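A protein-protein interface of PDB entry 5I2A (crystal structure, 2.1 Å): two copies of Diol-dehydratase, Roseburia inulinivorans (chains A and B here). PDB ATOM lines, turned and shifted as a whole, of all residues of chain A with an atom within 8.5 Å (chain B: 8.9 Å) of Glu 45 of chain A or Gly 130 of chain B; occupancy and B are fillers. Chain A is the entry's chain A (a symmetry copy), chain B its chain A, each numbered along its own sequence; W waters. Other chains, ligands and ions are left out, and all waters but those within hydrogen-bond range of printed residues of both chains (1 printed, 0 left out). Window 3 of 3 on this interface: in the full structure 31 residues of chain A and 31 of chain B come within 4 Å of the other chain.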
ATOM      1  N   THR A  38      -2.566 -16.204  28.010  1.00  0.00           N
ATOM      2  CA  THR A  38      -1.808 -17.276  27.382  1.00  0.00           C
ATOM      3  C   THR A  38      -2.576 -18.593  27.386  1.00  0.00           C
ATOM      4  O   THR A  38      -2.659 -19.281  26.384  1.00  0.00           O
ATOM      5  CB  THR A  38      -0.467 -17.465  28.079  1.00  0.00           C
ATOM      6  OG1 THR A  38       0.322 -16.294  27.873  1.00  0.00           O
ATOM      7  CG2 THR A  38       0.283 -18.661  27.519  1.00  0.00           C
ATOM      8  N   GLU A  39      -3.157 -18.922  28.525  1.00  0.00           N
ATOM      9  CA  GLU A  39      -3.995 -20.099  28.668  1.00  0.00           C
ATOM     10  C   GLU A  39      -5.148 -20.109  27.664  1.00  0.00           C
ATOM     11  O   GLU A  39      -5.422 -21.119  27.022  1.00  0.00           O
ATOM     12  CB  GLU A  39      -4.544 -20.146  30.083  1.00  0.00           C
ATOM     13  CG  GLU A  39      -4.979 -21.480  30.572  1.00  0.00           C
ATOM     14  CD  GLU A  39      -4.981 -21.508  32.088  1.00  0.00           C
ATOM     15  OE1 GLU A  39      -5.940 -20.993  32.697  1.00  0.00           O
ATOM     16  OE2 GLU A  39      -3.998 -22.013  32.665  1.00  0.00           O
ATOM     17  N   SER A  40      -5.830 -18.981  27.543  1.00  0.00           N
ATOM     18  CA  SER A  40      -6.955 -18.891  26.625  1.00  0.00           C
ATOM     19  C   SER A  40      -6.517 -18.991  25.160  1.00  0.00           C
ATOM     20  O   SER A  40      -7.097 -19.747  24.388  1.00  0.00           O
ATOM     21  CB  SER A  40      -7.723 -17.595  26.844  1.00  0.00           C
ATOM     22  OG  SER A  40      -8.860 -17.538  26.002  1.00  0.00           O
ATOM     23  N   PHE A  41      -5.504 -18.227  24.779  1.00  0.00           N
ATOM     24  CA  PHE A  41      -5.036 -18.243  23.390  1.00  0.00           C
ATOM     25  C   PHE A  41      -4.568 -19.643  22.941  1.00  0.00           C
ATOM     26  O   PHE A  41      -4.828 -20.054  21.812  1.00  0.00           O
ATOM     27  CB  PHE A  41      -3.922 -17.211  23.195  1.00  0.00           C
ATOM     28  CG  PHE A  41      -4.415 -15.914  22.600  1.00  0.00           C
ATOM     29  CD1 PHE A  41      -5.244 -15.078  23.328  1.00  0.00           C
ATOM     30  CD2 PHE A  41      -4.065 -15.549  21.308  1.00  0.00           C
ATOM     31  CE1 PHE A  41      -5.713 -13.887  22.773  1.00  0.00           C
ATOM     32  CE2 PHE A  41      -4.523 -14.370  20.749  1.00  0.00           C
ATOM     33  CZ  PHE A  41      -5.353 -13.539  21.482  1.00  0.00           C
ATOM     34  N   LYS A  42      -3.908 -20.376  23.831  1.00  0.00           N
ATOM     35  CA  LYS A  42      -3.527 -21.754  23.527  1.00  0.00           C
ATOM     36  C   LYS A  42      -4.756 -22.610  23.232  1.00  0.00           C
ATOM     37  O   LYS A  42      -4.682 -23.523  22.433  1.00  0.00           O
ATOM     38  CB  LYS A  42      -2.724 -22.372  24.676  1.00  0.00           C
ATOM     39  CG  LYS A  42      -1.298 -21.843  24.815  1.00  0.00           C
ATOM     40  CD  LYS A  42      -0.592 -22.475  26.035  1.00  0.00           C
ATOM     41  CE  LYS A  42       0.868 -22.060  26.106  1.00  0.00           C
ATOM     42  NZ  LYS A  42       1.527 -22.431  27.394  1.00  0.00           N
ATOM     43  N   ALA A  43      -5.885 -22.314  23.869  1.00  0.00           N
ATOM     44  CA  ALA A  43      -7.103 -23.091  23.643  1.00  0.00           C
ATOM     45  C   ALA A  43      -7.916 -22.661  22.420  1.00  0.00           C
ATOM     46  O   ALA A  43      -8.843 -23.354  22.024  1.00  0.00           O
ATOM     47  CB  ALA A  43      -7.997 -23.040  24.883  1.00  0.00           C
ATOM     48  N   THR A  44      -7.591 -21.524  21.824  1.00  0.00           N
ATOM     49  CA  THR A  44      -8.415 -21.027  20.731  1.00  0.00           C
ATOM     50  C   THR A  44      -7.667 -20.882  19.402  1.00  0.00           C
ATOM     51  O   THR A  44      -8.166 -20.233  18.495  1.00  0.00           O
ATOM     52  CB  THR A  44      -9.028 -19.652  21.075  1.00  0.00           C
ATOM     53  OG1 THR A  44      -7.977 -18.716  21.310  1.00  0.00           O
ATOM     54  CG2 THR A  44      -9.940 -19.743  22.303  1.00  0.00           C
ATOM     55  N   GLU A  45      -6.469 -21.450  19.306  1.00  0.00           N
ATOM     56  CA  GLU A  45      -5.683 -21.381  18.074  1.00  0.00           C
ATOM     57  C   GLU A  45      -6.520 -21.878  16.912  1.00  0.00           C
ATOM     58  O   GLU A  45      -7.216 -22.882  17.030  1.00  0.00           O
ATOM     59  CB  GLU A  45      -4.388 -22.198  18.196  1.00  0.00           C
ATOM     60  CG  GLU A  45      -3.367 -21.528  19.108  1.00  0.00           C
ATOM     61  CD  GLU A  45      -2.117 -22.349  19.344  1.00  0.00           C
ATOM     62  OE1 GLU A  45      -2.041 -23.511  18.888  1.00  0.00           O
ATOM     63  OE2 GLU A  45      -1.191 -21.815  19.976  1.00  0.00           O
ATOM     64  N   GLY A  46      -6.496 -21.141  15.811  1.00  0.00           N
ATOM     65  CA  GLY A  46      -7.242 -21.534  14.629  1.00  0.00           C
ATOM     66  C   GLY A  46      -8.541 -20.777  14.468  1.00  0.00           C
ATOM     67  O   GLY A  46      -9.150 -20.811  13.407  1.00  0.00           O
ATOM     68  N   GLN A  47      -8.974 -20.096  15.522  1.00  0.00           N
ATOM     69  CA  GLN A  47     -10.202 -19.311  15.475  1.00  0.00           C
ATOM     70  C   GLN A  47      -9.921 -17.864  15.047  1.00  0.00           C
ATOM     71  O   GLN A  47      -8.779 -17.423  15.102  1.00  0.00           O
ATOM     72  CB  GLN A  47     -10.891 -19.347  16.833  1.00  0.00           C
ATOM     73  CG  GLN A  47     -11.470 -20.712  17.187  1.00  0.00           C
ATOM     74  CD  GLN A  47     -12.116 -20.716  18.563  1.00  0.00           C
ATOM     75  OE1 GLN A  47     -12.953 -19.865  18.866  1.00  0.00           O
ATOM     76  NE2 GLN A  47     -11.718 -21.661  19.406  1.00  0.00           N
ATOM     77  N   PRO A  48     -10.958 -17.128  14.609  1.00  0.00           N
ATOM     78  CA  PRO A  48     -10.706 -15.743  14.198  1.00  0.00           C
ATOM     79  C   PRO A  48     -10.184 -14.913  15.366  1.00  0.00           C
ATOM     80  O   PRO A  48     -10.596 -15.139  16.508  1.00  0.00           O
ATOM     81  CB  PRO A  48     -12.086 -15.242  13.754  1.00  0.00           C
ATOM     82  CG  PRO A  48     -12.889 -16.476  13.508  1.00  0.00           C
ATOM     83  CD  PRO A  48     -12.385 -17.476  14.486  1.00  0.00           C
ATOM     84  N   ARG A  52     -10.942 -14.915  19.485  1.00  0.00           N
ATOM     85  CA  ARG A  52      -9.914 -15.273  20.451  1.00  0.00           C
ATOM     86  C   ARG A  52      -9.768 -14.186  21.525  1.00  0.00           C
ATOM     87  O   ARG A  52      -9.560 -14.514  22.695  1.00  0.00           O
ATOM     88  CB  ARG A  52      -8.579 -15.524  19.759  1.00  0.00           C
ATOM     89  CG  ARG A  52      -8.639 -16.672  18.725  1.00  0.00           C
ATOM     90  CD  ARG A  52      -7.270 -16.952  18.130  1.00  0.00           C
ATOM     91  NE  ARG A  52      -6.378 -17.624  19.068  1.00  0.00           N
ATOM     92  CZ  ARG A  52      -5.059 -17.706  18.912  1.00  0.00           C
ATOM     93  NH1 ARG A  52      -4.473 -17.138  17.868  1.00  0.00           N
ATOM     94  NH2 ARG A  52      -4.321 -18.348  19.804  1.00  0.00           N
ATOM     95  N   TYR A 127       5.086 -17.850  25.063  1.00  0.00           N
ATOM     96  CA  TYR A 127       4.041 -18.068  24.086  1.00  0.00           C
ATOM     97  C   TYR A 127       3.883 -16.909  23.094  1.00  0.00           C
ATOM     98  O   TYR A 127       3.518 -17.124  21.939  1.00  0.00           O
ATOM     99  CB  TYR A 127       2.703 -18.302  24.787  1.00  0.00           C
ATOM    100  CG  TYR A 127       1.578 -18.536  23.802  1.00  0.00           C
ATOM    101  CD1 TYR A 127       1.440 -19.760  23.153  1.00  0.00           C
ATOM    102  CD2 TYR A 127       0.680 -17.527  23.499  1.00  0.00           C
ATOM    103  CE1 TYR A 127       0.423 -19.975  22.241  1.00  0.00           C
ATOM    104  CE2 TYR A 127      -0.327 -17.724  22.591  1.00  0.00           C
ATOM    105  CZ  TYR A 127      -0.457 -18.954  21.971  1.00  0.00           C
ATOM    106  OH  TYR A 127      -1.473 -19.144  21.085  1.00  0.00           O
ATOM    107  N   LYS A 131       4.184 -13.157  18.321  1.00  0.00           N
ATOM    108  CA  LYS A 131       2.739 -12.958  18.236  1.00  0.00           C
ATOM    109  C   LYS A 131       2.283 -11.575  18.699  1.00  0.00           C
ATOM    110  O   LYS A 131       1.081 -11.327  18.808  1.00  0.00           O
ATOM    111  CB  LYS A 131       1.992 -14.015  19.070  1.00  0.00           C
ATOM    112  CG  LYS A 131       2.263 -15.477  18.707  1.00  0.00           C
ATOM    113  CD  LYS A 131       1.341 -16.412  19.517  1.00  0.00           C
ATOM    114  CE  LYS A 131       1.531 -17.868  19.146  1.00  0.00           C
ATOM    115  NZ  LYS A 131       2.924 -18.327  19.415  1.00  0.00           N
ATOM    116  N   PRO B  89       0.363 -28.535   4.184  1.00  0.00           N
ATOM    117  CA  PRO B  89      -0.247 -28.471   5.516  1.00  0.00           C
ATOM    118  C   PRO B  89      -0.799 -27.088   5.865  1.00  0.00           C
ATOM    119  O   PRO B  89      -1.563 -26.988   6.822  1.00  0.00           O
ATOM    120  CB  PRO B  89       0.914 -28.838   6.454  1.00  0.00           C
ATOM    121  CG  PRO B  89       2.132 -28.416   5.721  1.00  0.00           C
ATOM    122  CD  PRO B  89       1.822 -28.726   4.258  1.00  0.00           C
ATOM    123  N   GLU B  90      -0.426 -26.050   5.119  1.00  0.00           N
ATOM    124  CA  GLU B  90      -0.968 -24.712   5.371  1.00  0.00           C
ATOM    125  C   GLU B  90      -2.490 -24.694   5.155  1.00  0.00           C
ATOM    126  O   GLU B  90      -3.190 -23.847   5.702  1.00  0.00           O
ATOM    127  CB  GLU B  90      -0.289 -23.654   4.486  1.00  0.00           C
ATOM    128  CG  GLU B  90      -0.573 -23.763   2.985  1.00  0.00           C
ATOM    129  CD  GLU B  90       0.511 -24.529   2.214  1.00  0.00           C
ATOM    130  OE1 GLU B  90       0.848 -24.126   1.085  1.00  0.00           O
ATOM    131  OE2 GLU B  90       1.019 -25.536   2.739  1.00  0.00           O
ATOM    132  N   TYR B  93      -4.092 -31.033   6.907  1.00  0.00           N
ATOM    133  CA  TYR B  93      -3.221 -32.207   6.954  1.00  0.00           C
ATOM    134  C   TYR B  93      -3.791 -33.361   7.775  1.00  0.00           C
ATOM    135  O   TYR B  93      -3.337 -34.488   7.628  1.00  0.00           O
ATOM    136  CB  TYR B  93      -1.854 -31.834   7.518  1.00  0.00           C
ATOM    137  CG  TYR B  93      -1.923 -31.451   8.971  1.00  0.00           C
ATOM    138  CD1 TYR B  93      -1.848 -32.421   9.970  1.00  0.00           C
ATOM    139  CD2 TYR B  93      -2.082 -30.120   9.350  1.00  0.00           C
ATOM    140  CE1 TYR B  93      -1.928 -32.080  11.317  1.00  0.00           C
ATOM    141  CE2 TYR B  93      -2.159 -29.765  10.701  1.00  0.00           C
ATOM    142  CZ  TYR B  93      -2.081 -30.748  11.671  1.00  0.00           C
ATOM    143  OH  TYR B  93      -2.159 -30.416  12.998  1.00  0.00           O
ATOM    144  N   GLU B  94      -4.740 -33.085   8.670  1.00  0.00           N
ATOM    145  CA  GLU B  94      -5.239 -34.141   9.533  1.00  0.00           C
ATOM    146  C   GLU B  94      -5.830 -35.291   8.714  1.00  0.00           C
ATOM    147  O   GLU B  94      -5.692 -36.439   9.108  1.00  0.00           O
ATOM    148  CB  GLU B  94      -6.269 -33.605  10.539  1.00  0.00           C
ATOM    149  CG  GLU B  94      -5.602 -32.860  11.699  1.00  0.00           C
ATOM    150  CD  GLU B  94      -6.574 -32.302  12.727  1.00  0.00           C
ATOM    151  OE1 GLU B  94      -7.787 -32.560  12.629  1.00  0.00           O
ATOM    152  OE2 GLU B  94      -6.112 -31.599  13.645  1.00  0.00           O
ATOM    153  N   ASP B 125       3.918 -31.480  10.351  1.00  0.00           N
ATOM    154  CA  ASP B 125       2.513 -31.092  10.447  1.00  0.00           C
ATOM    155  C   ASP B 125       2.154 -30.489  11.812  1.00  0.00           C
ATOM    156  O   ASP B 125       1.255 -29.655  11.909  1.00  0.00           O
ATOM    157  CB  ASP B 125       1.585 -32.283  10.215  1.00  0.00           C
ATOM    158  CG  ASP B 125       1.589 -32.797   8.780  1.00  0.00           C
ATOM    159  OD1 ASP B 125       2.066 -32.115   7.860  1.00  0.00           O
ATOM    160  OD2 ASP B 125       1.089 -33.918   8.588  1.00  0.00           O
ATOM    161  N   ALA B 126       2.829 -30.945  12.867  1.00  0.00           N
ATOM    162  CA  ALA B 126       2.465 -30.547  14.219  1.00  0.00           C
ATOM    163  C   ALA B 126       2.471 -29.031  14.364  1.00  0.00           C
ATOM    164  O   ALA B 126       1.682 -28.474  15.104  1.00  0.00           O
ATOM    165  CB  ALA B 126       3.404 -31.185  15.246  1.00  0.00           C
ATOM    166  N   TYR B 127       3.363 -28.380  13.634  1.00  0.00           N
ATOM    167  CA  TYR B 127       3.446 -26.935  13.627  1.00  0.00           C
ATOM    168  C   TYR B 127       2.161 -26.253  13.139  1.00  0.00           C
ATOM    169  O   TYR B 127       1.833 -25.155  13.584  1.00  0.00           O
ATOM    170  CB  TYR B 127       4.610 -26.478  12.747  1.00  0.00           C
ATOM    171  CG  TYR B 127       4.736 -24.971  12.708  1.00  0.00           C
ATOM    172  CD1 TYR B 127       5.286 -24.273  13.780  1.00  0.00           C
ATOM    173  CD2 TYR B 127       4.277 -24.248  11.621  1.00  0.00           C
ATOM    174  CE1 TYR B 127       5.391 -22.895  13.757  1.00  0.00           C
ATOM    175  CE2 TYR B 127       4.367 -22.881  11.589  1.00  0.00           C
ATOM    176  CZ  TYR B 127       4.934 -22.209  12.657  1.00  0.00           C
ATOM    177  OH  TYR B 127       5.036 -20.853  12.605  1.00  0.00           O
ATOM    178  N   TRP B 128       1.455 -26.907  12.218  1.00  0.00           N
ATOM    179  CA  TRP B 128       0.335 -26.284  11.516  1.00  0.00           C
ATOM    180  C   TRP B 128      -0.983 -26.446  12.249  1.00  0.00           C
ATOM    181  O   TRP B 128      -1.987 -25.862  11.854  1.00  0.00           O
ATOM    182  CB  TRP B 128       0.245 -26.829  10.074  1.00  0.00           C
ATOM    183  CG  TRP B 128       1.401 -26.288   9.310  1.00  0.00           C
ATOM    184  CD1 TRP B 128       2.616 -26.891   9.120  1.00  0.00           C
ATOM    185  CD2 TRP B 128       1.499 -24.988   8.715  1.00  0.00           C
ATOM    186  NE1 TRP B 128       3.448 -26.055   8.428  1.00  0.00           N
ATOM    187  CE2 TRP B 128       2.789 -24.878   8.168  1.00  0.00           C
ATOM    188  CE3 TRP B 128       0.616 -23.908   8.584  1.00  0.00           C
ATOM    189  CZ2 TRP B 128       3.219 -23.740   7.499  1.00  0.00           C
ATOM    190  CZ3 TRP B 128       1.040 -22.783   7.919  1.00  0.00           C
ATOM    191  CH2 TRP B 128       2.335 -22.706   7.381  1.00  0.00           C
ATOM    192  N   LYS B 129      -0.970 -27.219  13.331  1.00  0.00           N
ATOM    193  CA  LYS B 129      -2.153 -27.354  14.174  1.00  0.00           C
ATOM    194  C   LYS B 129      -2.596 -25.972  14.645  1.00  0.00           C
ATOM    195  O   LYS B 129      -1.810 -25.227  15.195  1.00  0.00           O
ATOM    196  CB  LYS B 129      -1.871 -28.261  15.370  1.00  0.00           C
ATOM    197  CG  LYS B 129      -3.047 -28.428  16.313  1.00  0.00           C
ATOM    198  CD  LYS B 129      -4.205 -29.108  15.613  1.00  0.00           C
ATOM    199  CE  LYS B 129      -5.304 -29.493  16.606  1.00  0.00           C
ATOM    200  NZ  LYS B 129      -6.425 -30.216  15.939  1.00  0.00           N
ATOM    201  N   GLY B 130      -3.851 -25.625  14.398  1.00  0.00           N
ATOM    202  CA  GLY B 130      -4.336 -24.300  14.731  1.00  0.00           C
ATOM    203  C   GLY B 130      -3.848 -23.175  13.823  1.00  0.00           C
ATOM    204  O   GLY B 130      -4.030 -22.010  14.149  1.00  0.00           O
ATOM    205  N   LYS B 131      -3.239 -23.500  12.688  1.00  0.00           N
ATOM    206  CA  LYS B 131      -2.766 -22.460  11.778  1.00  0.00           C
ATOM    207  C   LYS B 131      -3.259 -22.632  10.342  1.00  0.00           C
ATOM    208  O   LYS B 131      -2.822 -21.904   9.449  1.00  0.00           O
ATOM    209  CB  LYS B 131      -1.227 -22.413  11.755  1.00  0.00           C
ATOM    210  CG  LYS B 131      -0.538 -22.175  13.101  1.00  0.00           C
ATOM    211  CD  LYS B 131       0.983 -22.004  12.904  1.00  0.00           C
ATOM    212  CE  LYS B 131       1.700 -21.705  14.204  1.00  0.00           C
ATOM    213  NZ  LYS B 131       1.533 -22.810  15.192  1.00  0.00           N
ATOM    214  N   THR B 132      -4.127 -23.612  10.102  1.00  0.00           N
ATOM    215  CA  THR B 132      -4.513 -23.948   8.733  1.00  0.00           C
ATOM    216  C   THR B 132      -5.661 -23.062   8.242  1.00  0.00           C
ATOM    217  O   THR B 132      -6.440 -22.538   9.047  1.00  0.00           O
ATOM    218  CB  THR B 132      -4.949 -25.420   8.614  1.00  0.00           C
ATOM    219  OG1 THR B 132      -6.102 -25.629   9.435  1.00  0.00           O
ATOM    220  CG2 THR B 132      -3.844 -26.364   9.064  1.00  0.00           C
ATOM    221  N   THR B 133      -5.784 -22.917   6.925  1.00  0.00           N
ATOM    222  CA  THR B 133      -6.936 -22.224   6.376  1.00  0.00           C
ATOM    223  C   THR B 133      -8.199 -22.987   6.720  1.00  0.00           C
ATOM    224  O   THR B 133      -9.218 -22.384   7.036  1.00  0.00           O
ATOM    225  CB  THR B 133      -6.846 -22.041   4.843  1.00  0.00           C
ATOM    226  OG1 THR B 133      -6.689 -23.315   4.199  1.00  0.00           O
ATOM    227  CG2 THR B 133      -5.686 -21.127   4.486  1.00  0.00           C
ATOM    228  N   SER B 134      -8.128 -24.320   6.682  1.00  0.00           N
ATOM    229  CA  SER B 134      -9.328 -25.122   6.860  1.00  0.00           C
ATOM    230  C   SER B 134      -9.943 -24.900   8.245  1.00  0.00           C
ATOM    231  O   SER B 134     -11.158 -24.827   8.374  1.00  0.00           O
ATOM    232  CB  SER B 134      -9.043 -26.615   6.630  1.00  0.00           C
ATOM    233  OG  SER B 134      -8.084 -27.114   7.531  1.00  0.00           O
ATOM    234  N   GLU B 135      -9.104 -24.765   9.267  1.00  0.00           N
ATOM    235  CA  GLU B 135      -9.607 -24.531  10.627  1.00  0.00           C
ATOM    236  C   GLU B 135     -10.240 -23.144  10.781  1.00  0.00           C
ATOM    237  O   GLU B 135     -11.290 -23.009  11.393  1.00  0.00           O
ATOM    238  CB  GLU B 135      -8.486 -24.709  11.656  1.00  0.00           C
ATOM    239  CG  GLU B 135      -8.104 -26.164  11.899  1.00  0.00           C
ATOM    240  CD  GLU B 135      -6.786 -26.301  12.652  1.00  0.00           C
ATOM    241  OE1 GLU B 135      -6.819 -26.526  13.874  1.00  0.00           O
ATOM    242  OE2 GLU B 135      -5.723 -26.149  12.029  1.00  0.00           O
ATOM    243  N   LEU B 136      -9.603 -22.116  10.233  1.00  0.00           N
ATOM    244  CA  LEU B 136     -10.203 -20.784  10.259  1.00  0.00           C
ATOM    245  C   LEU B 136     -11.517 -20.758   9.473  1.00  0.00           C
ATOM    246  O   LEU B 136     -12.497 -20.177   9.918  1.00  0.00           O
ATOM    247  CB  LEU B 136      -9.228 -19.737   9.710  1.00  0.00           C
ATOM    248  CG  LEU B 136      -9.733 -18.292   9.723  1.00  0.00           C
ATOM    249  CD1 LEU B 136     -10.113 -17.878  11.150  1.00  0.00           C
ATOM    250  CD2 LEU B 136      -8.684 -17.331   9.149  1.00  0.00           C
ATOM    251  N   SER B 139     -14.407 -22.187  11.552  1.00  0.00           N
ATOM    252  CA  SER B 139     -14.876 -21.271  12.589  1.00  0.00           C
ATOM    253  C   SER B 139     -15.747 -20.162  12.006  1.00  0.00           C
ATOM    254  O   SER B 139     -16.575 -19.598  12.701  1.00  0.00           O
ATOM    255  CB  SER B 139     -13.690 -20.662  13.347  1.00  0.00           C
ATOM    256  OG  SER B 139     -12.886 -21.673  13.922  1.00  0.00           O
ATOM    257  N   LEU B 521      -5.024 -15.931   5.567  1.00  0.00           N
ATOM    258  CA  LEU B 521      -3.900 -16.794   5.882  1.00  0.00           C
ATOM    259  C   LEU B 521      -3.074 -17.227   4.666  1.00  0.00           C
ATOM    260  O   LEU B 521      -1.927 -17.612   4.816  1.00  0.00           O
ATOM    261  CB  LEU B 521      -4.400 -18.033   6.642  1.00  0.00           C
ATOM    262  CG  LEU B 521      -4.984 -17.777   8.040  1.00  0.00           C
ATOM    263  CD1 LEU B 521      -5.472 -19.080   8.686  1.00  0.00           C
ATOM    264  CD2 LEU B 521      -3.947 -17.087   8.944  1.00  0.00           C
HETATM  265  O   HOH W   1      -4.636 -19.029  15.071  1.00  0.00           O
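The backbone NH (N) of Gly 46 of chain A sits at hydrogen-bond distance from the backbone carbonyl oxygen (O) of Gly 130 of chain B (3.1 Å). The backbone NH of Leu 136 of chain B lies close to the backbone carbonyl oxygen of Gly 46 of chain A (3.5 Å).
Positions printed for both chains: 127 and 131. Of the 9 pairs that touch across the chains among the printed residues, none has its exchanged pair printed and touching as well.
Glu 45 of chain A touches one residue of chain B. Of the printed residues of chain B, Gln 47 of chain A touches Leu 136 (3.9 Å) and Ser 139 (3.7 Å). Gly 130 of chain B touches just these residues of chain A: Glu 45 and Gly 46. Ser 134 of chain B touches none of the printed residues of chain A. Of the printed residues of chain A, Leu 136 of chain B touches Gly 46 (3.3 Å), Gln 47 (3.9 Å) and Pro 48 (3.6 Å). The nearest residue of chain B that does not touch Glu 45 of chain A is Lys 129 of chain B (4.1 Å).
Water W1 lies within hydrogen-bond range of the backbone NH of Gly 46 of chain A (2.9 Å), the backbone carbonyl oxygen of Gly 130 of chain B (3.2 Å) and the guanidinium group of Arg 52 of chain A (3.4 Å).
Printed residues of chain B that touch a printed residue of chain A: Gly 130, Glu 135, Leu 136 and Ser 139. Hydrophobic or aromatic side chains of chain B that line the printed part of chain A: Leu 136. Of the 14 printed residues of chain A, 4 touch a printed residue of chain B.
O of Gly 130 of chain B touches C of Glu 45 of chain A (3.7 Å). Gly 46 of chain A touches Glu 135 of chain B (O to O, 3.7 Å). Ser 139 of chain B touches Gly 46 of chain A (OG to O, 3.9 Å). Gln 47 of chain A touches Leu 136 of chain B. Gln 47 of chain A touches Ser 139 of chain B. Pro 48 of chain A touches Leu 136 of chain B. Ser 139 of chain B touches Pro 48 of chain A (CB to CD, 3.6 Å).
The side-chain carboxylate (OE2) of Glu 45 of chain A sits at hydrogen-bond distance from the side-chain hydroxyl (OH) of Tyr 127 of chain A. The side-chain carboxylate (OE2) of Glu 135 of chain B sits at hydrogen-bond distance from the backbone NH (N) of Gly 130 of chain B. The side-chain hydroxyl (OG1) of Thr 132 of chain B is in hydrogen-bond range of the side-chain carboxylate (OE2) of Glu 135 of chain B. The backbone carbonyl oxygen of Glu 135 of chain B lies within hydrogen-bond range of the side-chain hydroxyl of Ser 139 of chain B, 3.3 Å away.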
